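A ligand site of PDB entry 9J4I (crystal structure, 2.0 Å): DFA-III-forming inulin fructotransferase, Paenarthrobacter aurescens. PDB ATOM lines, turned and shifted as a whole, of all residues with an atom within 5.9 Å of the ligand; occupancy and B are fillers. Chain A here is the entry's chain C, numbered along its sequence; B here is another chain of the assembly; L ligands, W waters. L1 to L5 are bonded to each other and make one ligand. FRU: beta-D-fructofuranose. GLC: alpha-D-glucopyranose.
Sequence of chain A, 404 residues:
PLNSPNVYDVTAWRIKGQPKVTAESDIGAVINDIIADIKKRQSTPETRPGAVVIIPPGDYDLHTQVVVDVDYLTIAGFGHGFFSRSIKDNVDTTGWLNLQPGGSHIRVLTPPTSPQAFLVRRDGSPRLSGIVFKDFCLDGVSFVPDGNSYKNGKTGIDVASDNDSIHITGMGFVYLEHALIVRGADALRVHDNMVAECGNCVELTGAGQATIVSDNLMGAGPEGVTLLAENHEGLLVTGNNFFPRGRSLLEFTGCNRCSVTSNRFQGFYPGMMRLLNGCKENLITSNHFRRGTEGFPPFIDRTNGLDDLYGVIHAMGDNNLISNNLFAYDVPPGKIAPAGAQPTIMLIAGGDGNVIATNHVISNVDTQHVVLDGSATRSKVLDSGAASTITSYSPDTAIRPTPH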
ATOM      1  N   ARG A 257      -6.318  -8.912   2.862  1.00  0.00           N
ATOM      2  CA  ARG A 257      -7.544  -9.702   2.556  1.00  0.00           C
ATOM      3  C   ARG A 257      -7.171 -10.725   1.495  1.00  0.00           C
ATOM      4  O   ARG A 257      -7.952 -10.917   0.518  1.00  0.00           O
ATOM      5  CB  ARG A 257      -8.664  -8.724   2.214  1.00  0.00           C
ATOM      6  CG  ARG A 257      -9.093  -7.882   3.416  1.00  0.00           C
ATOM      7  CD  ARG A 257      -9.970  -6.698   3.047  1.00  0.00           C
ATOM      8  NE  ARG A 257      -9.283  -5.637   2.323  1.00  0.00           N
ATOM      9  CZ  ARG A 257      -8.599  -4.649   2.879  1.00  0.00           C
ATOM     10  NH1 ARG A 257      -8.494  -4.537   4.197  1.00  0.00           N
ATOM     11  NH2 ARG A 257      -8.027  -3.749   2.113  1.00  0.00           N
ATOM     12  N   LYS A 280      -2.784  -6.851   6.301  1.00  0.00           N
ATOM     13  CA  LYS A 280      -4.003  -6.903   7.156  1.00  0.00           C
ATOM     14  C   LYS A 280      -4.949  -7.998   6.669  1.00  0.00           C
ATOM     15  O   LYS A 280      -5.130  -8.134   5.460  1.00  0.00           O
ATOM     16  CB  LYS A 280      -4.759  -5.579   7.141  1.00  0.00           C
ATOM     17  CG  LYS A 280      -3.982  -4.356   7.617  1.00  0.00           C
ATOM     18  CD  LYS A 280      -4.891  -3.179   7.892  1.00  0.00           C
ATOM     19  CE  LYS A 280      -4.145  -1.940   8.330  1.00  0.00           C
ATOM     20  NZ  LYS A 280      -5.046  -0.949   8.974  1.00  0.00           N
ATOM     21  N   GLU A 281      -5.594  -8.676   7.617  1.00  0.00           N
ATOM     22  CA  GLU A 281      -6.825  -9.469   7.375  1.00  0.00           C
ATOM     23  C   GLU A 281      -6.525 -10.584   6.377  1.00  0.00           C
ATOM     24  O   GLU A 281      -7.379 -10.878   5.533  1.00  0.00           O
ATOM     25  CB  GLU A 281      -7.951  -8.539   6.932  1.00  0.00           C
ATOM     26  CG  GLU A 281      -8.263  -7.467   7.966  1.00  0.00           C
ATOM     27  CD  GLU A 281      -8.963  -6.227   7.428  1.00  0.00           C
ATOM     28  OE1 GLU A 281      -9.634  -6.323   6.378  1.00  0.00           O
ATOM     29  OE2 GLU A 281      -8.853  -5.169   8.084  1.00  0.00           O
ATOM     30  N   GLY A 317       1.491  -6.932  10.830  1.00  0.00           N
ATOM     31  CA  GLY A 317       0.223  -6.362  10.332  1.00  0.00           C
ATOM     32  C   GLY A 317      -0.946  -6.724  11.219  1.00  0.00           C
ATOM     33  O   GLY A 317      -0.710  -7.300  12.273  1.00  0.00           O
ATOM     34  N   ASP A 318      -2.162  -6.340  10.815  1.00  0.00           N
ATOM     35  CA  ASP A 318      -3.367  -6.391  11.690  1.00  0.00           C
ATOM     36  C   ASP A 318      -4.244  -7.570  11.291  1.00  0.00           C
ATOM     37  O   ASP A 318      -4.424  -7.829  10.084  1.00  0.00           O
ATOM     38  CB  ASP A 318      -4.182  -5.099  11.602  1.00  0.00           C
ATOM     39  CG  ASP A 318      -3.426  -3.841  12.032  1.00  0.00           C
ATOM     40  OD1 ASP A 318      -2.365  -4.014  12.648  1.00  0.00           O
ATOM     41  OD2 ASP A 318      -3.926  -2.723  11.786  1.00  0.00           O
ATOM     42  N   ASN A 319      -4.809  -8.243  12.287  1.00  0.00           N
ATOM     43  CA  ASN A 319      -6.027  -9.074  12.128  1.00  0.00           C
ATOM     44  C   ASN A 319      -5.784 -10.230  11.141  1.00  0.00           C
ATOM     45  O   ASN A 319      -6.729 -10.604  10.433  1.00  0.00           O
ATOM     46  CB  ASN A 319      -7.195  -8.205  11.666  1.00  0.00           C
ATOM     47  CG  ASN A 319      -7.786  -7.412  12.808  1.00  0.00           C
ATOM     48  OD1 ASN A 319      -7.924  -6.189  12.722  1.00  0.00           O
ATOM     49  ND2 ASN A 319      -8.130  -8.117  13.868  1.00  0.00           N
ATOM     50  N   GLY A 351       1.620  -5.401  15.114  1.00  0.00           N
ATOM     51  CA  GLY A 351       0.258  -5.286  14.582  1.00  0.00           C
ATOM     52  C   GLY A 351      -0.780  -5.632  15.625  1.00  0.00           C
ATOM     53  O   GLY A 351      -0.429  -6.169  16.709  1.00  0.00           O
ATOM     54  N   ASP A 352      -2.025  -5.362  15.255  1.00  0.00           N
ATOM     55  CA  ASP A 352      -3.200  -5.354  16.157  1.00  0.00           C
ATOM     56  C   ASP A 352      -4.175  -6.468  15.759  1.00  0.00           C
ATOM     57  O   ASP A 352      -4.495  -6.567  14.560  1.00  0.00           O
ATOM     58  CB  ASP A 352      -3.848  -3.976  16.096  1.00  0.00           C
ATOM     59  CG  ASP A 352      -5.011  -3.841  17.037  1.00  0.00           C
ATOM     60  OD1 ASP A 352      -4.853  -4.148  18.239  1.00  0.00           O
ATOM     61  OD2 ASP A 352      -6.094  -3.479  16.545  1.00  0.00           O
ATOM     62  N   GLY A 353      -4.596  -7.276  16.732  1.00  0.00           N
ATOM     63  CA  GLY A 353      -5.723  -8.222  16.614  1.00  0.00           C
ATOM     64  C   GLY A 353      -5.339  -9.537  15.940  1.00  0.00           C
ATOM     65  O   GLY A 353      -6.255 -10.287  15.606  1.00  0.00           O
ATOM     66  N   THR A 377      -0.581  -5.767  19.772  1.00  0.00           N
ATOM     67  CA  THR A 377      -1.755  -5.389  20.602  1.00  0.00           C
ATOM     68  C   THR A 377      -2.892  -6.355  20.300  1.00  0.00           C
ATOM     69  O   THR A 377      -2.979  -6.851  19.137  1.00  0.00           O
ATOM     70  CB  THR A 377      -2.151  -3.914  20.408  1.00  0.00           C
ATOM     71  OG1 THR A 377      -2.376  -3.686  19.018  1.00  0.00           O
ATOM     72  CG2 THR A 377      -1.102  -2.937  20.892  1.00  0.00           C
ATOM     73  N   ARG A 378      -3.707  -6.607  21.313  1.00  0.00           N
ATOM     74  CA  ARG A 378      -4.972  -7.394  21.218  1.00  0.00           C
ATOM     75  C   ARG A 378      -4.760  -8.692  20.437  1.00  0.00           C
ATOM     76  O   ARG A 378      -5.672  -9.094  19.674  1.00  0.00           O
ATOM     77  CB  ARG A 378      -6.022  -6.476  20.602  1.00  0.00           C
ATOM     78  CG  ARG A 378      -6.159  -5.145  21.348  1.00  0.00           C
ATOM     79  CD  ARG A 378      -7.452  -4.436  21.044  1.00  0.00           C
ATOM     80  NE  ARG A 378      -7.386  -3.850  19.719  1.00  0.00           N
ATOM     81  CZ  ARG A 378      -8.319  -3.070  19.198  1.00  0.00           C
ATOM     82  NH1 ARG A 378      -9.415  -2.764  19.881  1.00  0.00           N
ATOM     83  NH2 ARG A 378      -8.156  -2.567  17.987  1.00  0.00           N
ATOM     84  N   ARG B 290     -14.915 -11.423   2.392  1.00  0.00           N
ATOM     85  CA  ARG B 290     -14.784  -9.948   2.442  1.00  0.00           C
ATOM     86  C   ARG B 290     -16.122  -9.336   2.011  1.00  0.00           C
ATOM     87  O   ARG B 290     -16.508  -9.495   0.832  1.00  0.00           O
ATOM     88  CB  ARG B 290     -13.625  -9.482   1.560  1.00  0.00           C
ATOM     89  CG  ARG B 290     -13.144  -8.076   1.851  1.00  0.00           C
ATOM     90  CD  ARG B 290     -14.146  -6.951   1.600  1.00  0.00           C
ATOM     91  NE  ARG B 290     -13.465  -5.684   1.705  1.00  0.00           N
ATOM     92  CZ  ARG B 290     -13.079  -5.105   2.843  1.00  0.00           C
ATOM     93  NH1 ARG B 290     -13.371  -5.631   4.019  1.00  0.00           N
ATOM     94  NH2 ARG B 290     -12.395  -3.962   2.786  1.00  0.00           N
ATOM     95  N   TYR B 329     -15.432  -7.400   7.208  1.00  0.00           N
ATOM     96  CA  TYR B 329     -16.630  -6.555   6.927  1.00  0.00           C
ATOM     97  C   TYR B 329     -16.222  -5.074   6.979  1.00  0.00           C
ATOM     98  O   TYR B 329     -15.838  -4.574   8.065  1.00  0.00           O
ATOM     99  CB  TYR B 329     -17.741  -6.882   7.922  1.00  0.00           C
ATOM    100  CG  TYR B 329     -19.052  -6.178   7.677  1.00  0.00           C
ATOM    101  CD1 TYR B 329     -19.231  -4.850   8.057  1.00  0.00           C
ATOM    102  CD2 TYR B 329     -20.125  -6.821   7.081  1.00  0.00           C
ATOM    103  CE1 TYR B 329     -20.425  -4.187   7.818  1.00  0.00           C
ATOM    104  CE2 TYR B 329     -21.327  -6.164   6.843  1.00  0.00           C
ATOM    105  CZ  TYR B 329     -21.477  -4.839   7.212  1.00  0.00           C
ATOM    106  OH  TYR B 329     -22.659  -4.187   7.000  1.00  0.00           O
ATOM    107  N   ASP B 330     -16.392  -4.367   5.873  1.00  0.00           N
ATOM    108  CA  ASP B 330     -16.174  -2.890   5.848  1.00  0.00           C
ATOM    109  C   ASP B 330     -17.244  -2.246   4.974  1.00  0.00           C
ATOM    110  O   ASP B 330     -17.077  -2.218   3.751  1.00  0.00           O
ATOM    111  CB  ASP B 330     -14.785  -2.513   5.342  1.00  0.00           C
ATOM    112  CG  ASP B 330     -14.400  -1.063   5.596  1.00  0.00           C
ATOM    113  OD1 ASP B 330     -15.254  -0.292   6.083  1.00  0.00           O
ATOM    114  OD2 ASP B 330     -13.228  -0.717   5.363  1.00  0.00           O
ATOM    115  N   VAL B 331     -18.301  -1.747   5.603  1.00  0.00           N
ATOM    116  CA  VAL B 331     -19.440  -1.050   4.932  1.00  0.00           C
ATOM    117  C   VAL B 331     -19.635   0.282   5.648  1.00  0.00           C
ATOM    118  O   VAL B 331     -19.783   0.279   6.877  1.00  0.00           O
ATOM    119  CB  VAL B 331     -20.719  -1.915   4.971  1.00  0.00           C
ATOM    120  CG1 VAL B 331     -21.878  -1.246   4.244  1.00  0.00           C
ATOM    121  CG2 VAL B 331     -20.482  -3.297   4.397  1.00  0.00           C
ATOM    122  N   PRO B 332     -19.649   1.427   4.940  1.00  0.00           N
ATOM    123  CA  PRO B 332     -19.915   2.727   5.578  1.00  0.00           C
ATOM    124  C   PRO B 332     -21.222   2.676   6.351  1.00  0.00           C
ATOM    125  O   PRO B 332     -22.209   2.099   5.882  1.00  0.00           O
ATOM    126  CB  PRO B 332     -19.961   3.712   4.404  1.00  0.00           C
ATOM    127  CG  PRO B 332     -19.172   3.047   3.301  1.00  0.00           C
ATOM    128  CD  PRO B 332     -19.430   1.570   3.487  1.00  0.00           C
ATOM    129  N   ILE B 362     -13.409  -9.238  11.492  1.00  0.00           N
ATOM    130  CA  ILE B 362     -13.029  -7.801  11.546  1.00  0.00           C
ATOM    131  C   ILE B 362     -14.211  -7.033  10.975  1.00  0.00           C
ATOM    132  O   ILE B 362     -14.698  -7.403   9.871  1.00  0.00           O
ATOM    133  CB  ILE B 362     -11.751  -7.495  10.723  1.00  0.00           C
ATOM    134  CG1 ILE B 362     -10.642  -8.512  11.008  1.00  0.00           C
ATOM    135  CG2 ILE B 362     -11.290  -6.059  10.946  1.00  0.00           C
ATOM    136  CD1 ILE B 362     -10.657  -9.703  10.072  1.00  0.00           C
ATOM    137  N   SER B 363     -14.680  -6.025  11.690  1.00  0.00           N
ATOM    138  CA  SER B 363     -15.684  -5.093  11.126  1.00  0.00           C
ATOM    139  C   SER B 363     -15.357  -3.669  11.535  1.00  0.00           C
ATOM    140  O   SER B 363     -14.784  -3.474  12.615  1.00  0.00           O
ATOM    141  CB  SER B 363     -17.092  -5.473  11.535  1.00  0.00           C
ATOM    142  OG  SER B 363     -17.148  -5.609  12.947  1.00  0.00           O
ATOM    143  N   ASN B 364     -15.739  -2.728  10.677  1.00  0.00           N
ATOM    144  CA  ASN B 364     -15.626  -1.262  10.878  1.00  0.00           C
ATOM    145  C   ASN B 364     -16.708  -0.748  11.846  1.00  0.00           C
ATOM    146  O   ASN B 364     -16.551   0.363  12.348  1.00  0.00           O
ATOM    147  CB  ASN B 364     -15.679  -0.559   9.522  1.00  0.00           C
ATOM    148  CG  ASN B 364     -17.046  -0.694   8.866  1.00  0.00           C
ATOM    149  OD1 ASN B 364     -17.563  -1.790   8.692  1.00  0.00           O
ATOM    150  ND2 ASN B 364     -17.631   0.433   8.496  1.00  0.00           N
HETATM  151  C1  FRU L   1     -10.114   4.037   6.806  1.00  0.00           C
HETATM  152  C2  FRU L   1     -11.013   2.945   7.383  1.00  0.00           C
HETATM  153  C3  FRU L   1     -12.340   2.642   6.687  1.00  0.00           C
HETATM  154  C4  FRU L   1     -13.057   1.861   7.782  1.00  0.00           C
HETATM  155  C5  FRU L   1     -12.687   2.578   9.056  1.00  0.00           C
HETATM  156  C6  FRU L   1     -12.596   1.553  10.188  1.00  0.00           C
HETATM  157  O1  FRU L   1     -10.706   5.302   7.011  1.00  0.00           O
HETATM  158  O3  FRU L   1     -12.290   1.849   5.474  1.00  0.00           O
HETATM  159  O4  FRU L   1     -14.476   1.838   7.671  1.00  0.00           O
HETATM  160  O5  FRU L   1     -11.447   3.262   8.729  1.00  0.00           O
HETATM  161  O6  FRU L   1     -12.710   2.154  11.493  1.00  0.00           O
HETATM  162  C1  FRU L   2      -9.043   1.672   8.368  1.00  0.00           C
HETATM  163  C2  FRU L   2      -8.919   0.165   8.643  1.00  0.00           C
HETATM  164  C3  FRU L   2      -8.571  -0.635   7.388  1.00  0.00           C
HETATM  165  C4  FRU L   2      -8.972  -2.038   7.765  1.00  0.00           C
HETATM  166  C5  FRU L   2     -10.272  -1.738   8.493  1.00  0.00           C
HETATM  167  C6  FRU L   2     -10.556  -2.702   9.622  1.00  0.00           C
HETATM  168  O1  FRU L   2     -10.044   2.002   7.409  1.00  0.00           O
HETATM  169  O3  FRU L   2      -7.200  -0.465   7.032  1.00  0.00           O
HETATM  170  O4  FRU L   2      -9.075  -2.920   6.638  1.00  0.00           O
HETATM  171  O5  FRU L   2     -10.172  -0.394   9.012  1.00  0.00           O
HETATM  172  O6  FRU L   2     -11.775  -2.450  10.332  1.00  0.00           O
HETATM  173  C1  FRU L   3      -8.395   0.177  11.040  1.00  0.00           C
HETATM  174  C2  FRU L   3      -7.304  -0.288  11.975  1.00  0.00           C
HETATM  175  C3  FRU L   3      -7.220  -1.825  12.083  1.00  0.00           C
HETATM  176  C4  FRU L   3      -6.691  -2.005  13.474  1.00  0.00           C
HETATM  177  C5  FRU L   3      -7.221  -0.790  14.219  1.00  0.00           C
HETATM  178  C6  FRU L   3      -6.097  -0.086  14.955  1.00  0.00           C
HETATM  179  O1  FRU L   3      -8.068  -0.050   9.674  1.00  0.00           O
HETATM  180  O3  FRU L   3      -6.381  -2.457  11.125  1.00  0.00           O
HETATM  181  O4  FRU L   3      -7.098  -3.261  14.036  1.00  0.00           O
HETATM  182  O5  FRU L   3      -7.768   0.116  13.251  1.00  0.00           O
HETATM  183  O6  FRU L   3      -6.662   1.013  15.642  1.00  0.00           O
HETATM  184  C1  FRU L   4      -5.848   1.624  11.693  1.00  0.00           C
HETATM  185  C2  FRU L   4      -4.418   1.978  11.274  1.00  0.00           C
HETATM  186  C3  FRU L   4      -4.283   3.504  11.254  1.00  0.00           C
HETATM  187  C4  FRU L   4      -3.670   3.787   9.902  1.00  0.00           C
HETATM  188  C5  FRU L   4      -4.223   2.652   9.054  1.00  0.00           C
HETATM  189  C6  FRU L   4      -3.431   2.497   7.778  1.00  0.00           C
HETATM  190  O1  FRU L   4      -6.076   0.208  11.764  1.00  0.00           O
HETATM  191  O2  FRU L   4      -3.522   1.354  12.191  1.00  0.00           O
HETATM  192  O3  FRU L   4      -3.572   4.060  12.360  1.00  0.00           O
HETATM  193  O4  FRU L   4      -4.063   5.004   9.284  1.00  0.00           O
HETATM  194  O5  FRU L   4      -4.167   1.537   9.944  1.00  0.00           O
HETATM  195  O6  FRU L   4      -3.862   1.305   7.141  1.00  0.00           O
HETATM  196  C1  GLC L   5      -2.108   1.386  12.010  1.00  0.00           C
HETATM  197  C2  GLC L   5      -1.529  -0.011  12.179  1.00  0.00           C
HETATM  198  C3  GLC L   5      -1.874  -0.564  13.552  1.00  0.00           C
HETATM  199  C4  GLC L   5      -1.418   0.428  14.613  1.00  0.00           C
HETATM  200  C5  GLC L   5      -2.006   1.814  14.395  1.00  0.00           C
HETATM  201  C6  GLC L   5      -1.419   2.830  15.363  1.00  0.00           C
HETATM  202  O2  GLC L   5      -2.052  -0.878  11.159  1.00  0.00           O
HETATM  203  O3  GLC L   5      -1.253  -1.844  13.692  1.00  0.00           O
HETATM  204  O4  GLC L   5      -1.801  -0.061  15.900  1.00  0.00           O
HETATM  205  O5  GLC L   5      -1.714   2.266  13.074  1.00  0.00           O
HETATM  206  O6  GLC L   5      -0.011   2.944  15.022  1.00  0.00           O
HETATM  207  O   HOH W   1       1.899  -1.771  12.993  1.00  0.00           O
HETATM  208  O   HOH W   2     -11.290  -2.247   4.853  1.00  0.00           O
HETATM  209  O   HOH W   3      -7.030  -2.080   4.647  1.00  0.00           O
HETATM  210  O   HOH W   4     -13.253  -3.990   8.523  1.00  0.00           O
HETATM  211  O   HOH W   5      -6.708   1.922   5.536  1.00  0.00           O
HETATM  212  O   HOH W   6       0.140   0.298  18.763  1.00  0.00           O
HETATM  213  O   HOH W   7     -11.543  -2.881  12.718  1.00  0.00           O
HETATM  214  O   HOH W   8     -11.838  -4.874   6.361  1.00  0.00           O
HETATM  215  O   HOH W   9      -7.429  -4.913  10.234  1.00  0.00           O
HETATM  216  O   HOH W  10      -0.781  -2.328  17.258  1.00  0.00           O
HETATM  217  O   HOH W  11     -16.263   3.163   9.096  1.00  0.00           O
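NZ of Lys 280 lies within hydrogen-bond range of O5 of FRU L4, at 2.8 Å. An oxygen (O4) of FRU L3 sits at hydrogen-bond distance from the side-chain carboxylate (OD2) of Asp 352, at 2.7 Å. The side-chain amide oxygen (OD1) of Asn 319 is in hydrogen-bond range of an oxygen (O4) of FRU L3 (3.3 Å). O3 of FRU L1 lies within hydrogen-bond range of OD2 of Asp 330 of chain B (2.7 Å). The side-chain carboxylate (OD2) of Asp 318 is in hydrogen-bond range of an oxygen (O3) of FRU L3 (2.6 Å). The guanidinium group (NH1) of Arg 257 lies within hydrogen-bond range of an oxygen (O4) of FRU L2, 3.0 Å away. The side-chain carboxylate of Glu 281 is in hydrogen-bond range of an oxygen (O4) of FRU L2 (2.7 Å).
CA of Gly 351 touches O3 of GLC L5, 3.9 Å away. CG2 of Ile 362 of chain B touches C6 of FRU L2 (3.7 Å). O of Ser 363 of chain B touches O6 of FRU L2, at 3.9 Å. CB of Asn 364 of chain B touches O4 of FRU L1, 3.3 Å away. Hydrophobic or aromatic side chains that line the ligand: Ile 362 of chain B. Of the 19 residues printed, 11 come within 4 Å of the ligand. The nearest printed residue that does not touch the ligand is Arg 378 (4.1 Å).
Water W7 lies within hydrogen-bond range of O6 of FRU L2 and O of Ser 363 of chain B. Water W4 bridges O of Tyr 329 of chain B (2.7 Å) and O6 of FRU L2 (2.8 Å). Water W9 lies within hydrogen-bond range of OE2 of Glu 281 (2.6 Å), O3 of FRU L3 (2.8 Å) and OD1 of Asn 319 (2.8 Å). Water W10 lies within hydrogen-bond range of the side-chain hydroxyl (OG1) of Thr 377 (2.7 Å) and an oxygen (O4) of GLC L5 (2.8 Å). Water W2 lies within hydrogen-bond range of the side-chain carboxylate of Asp 330 of chain B (2.5 Å), the guanidinium group of Arg 290 of chain B (2.9 Å) and an oxygen (O4) of FRU L2 (2.9 Å). Water W8 lies within hydrogen-bond range of the side-chain carboxylate (OE1) of Glu 281 (2.6 Å), the guanidinium group (NH1) of Arg 290 of chain B (2.9 Å) and an oxygen (O4) of FRU L2 (3.4 Å).
The backbone carbonyl oxygen (O) of Gly 351 lies within hydrogen-bond range of the backbone NH (N) of Thr 377, 3.1 Å away. The side-chain carboxylate (OE1) of Glu 281 is in salt-bridge range of the guanidinium group (NH1) of Arg 257 (3.0 Å). N of Asn 319 sits at hydrogen-bond distance from O of Asp 352 (2.8 Å). The side-chain carboxylate (OD1) of Asp 330 of chain B lies close to the side-chain amide nitrogen (ND2) of Asn 364 of chain B, 3.5 Å away. The side-chain amide nitrogen (ND2) of Asn 319 lies within hydrogen-bond range of the backbone carbonyl oxygen (O) of Gly 353. The backbone NH (N) of Arg 257 lies within hydrogen-bond range of the backbone carbonyl oxygen (O) of Lys 280 (3.0 Å). The side-chain carboxylate of Asp 352 is in salt-bridge range of the guanidinium group of Arg 378, 2.7 Å away. The backbone carbonyl oxygen (O) of Ile 362 of chain B sits at hydrogen-bond distance from the backbone NH (N) of Tyr 329 of chain B (2.8 Å).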
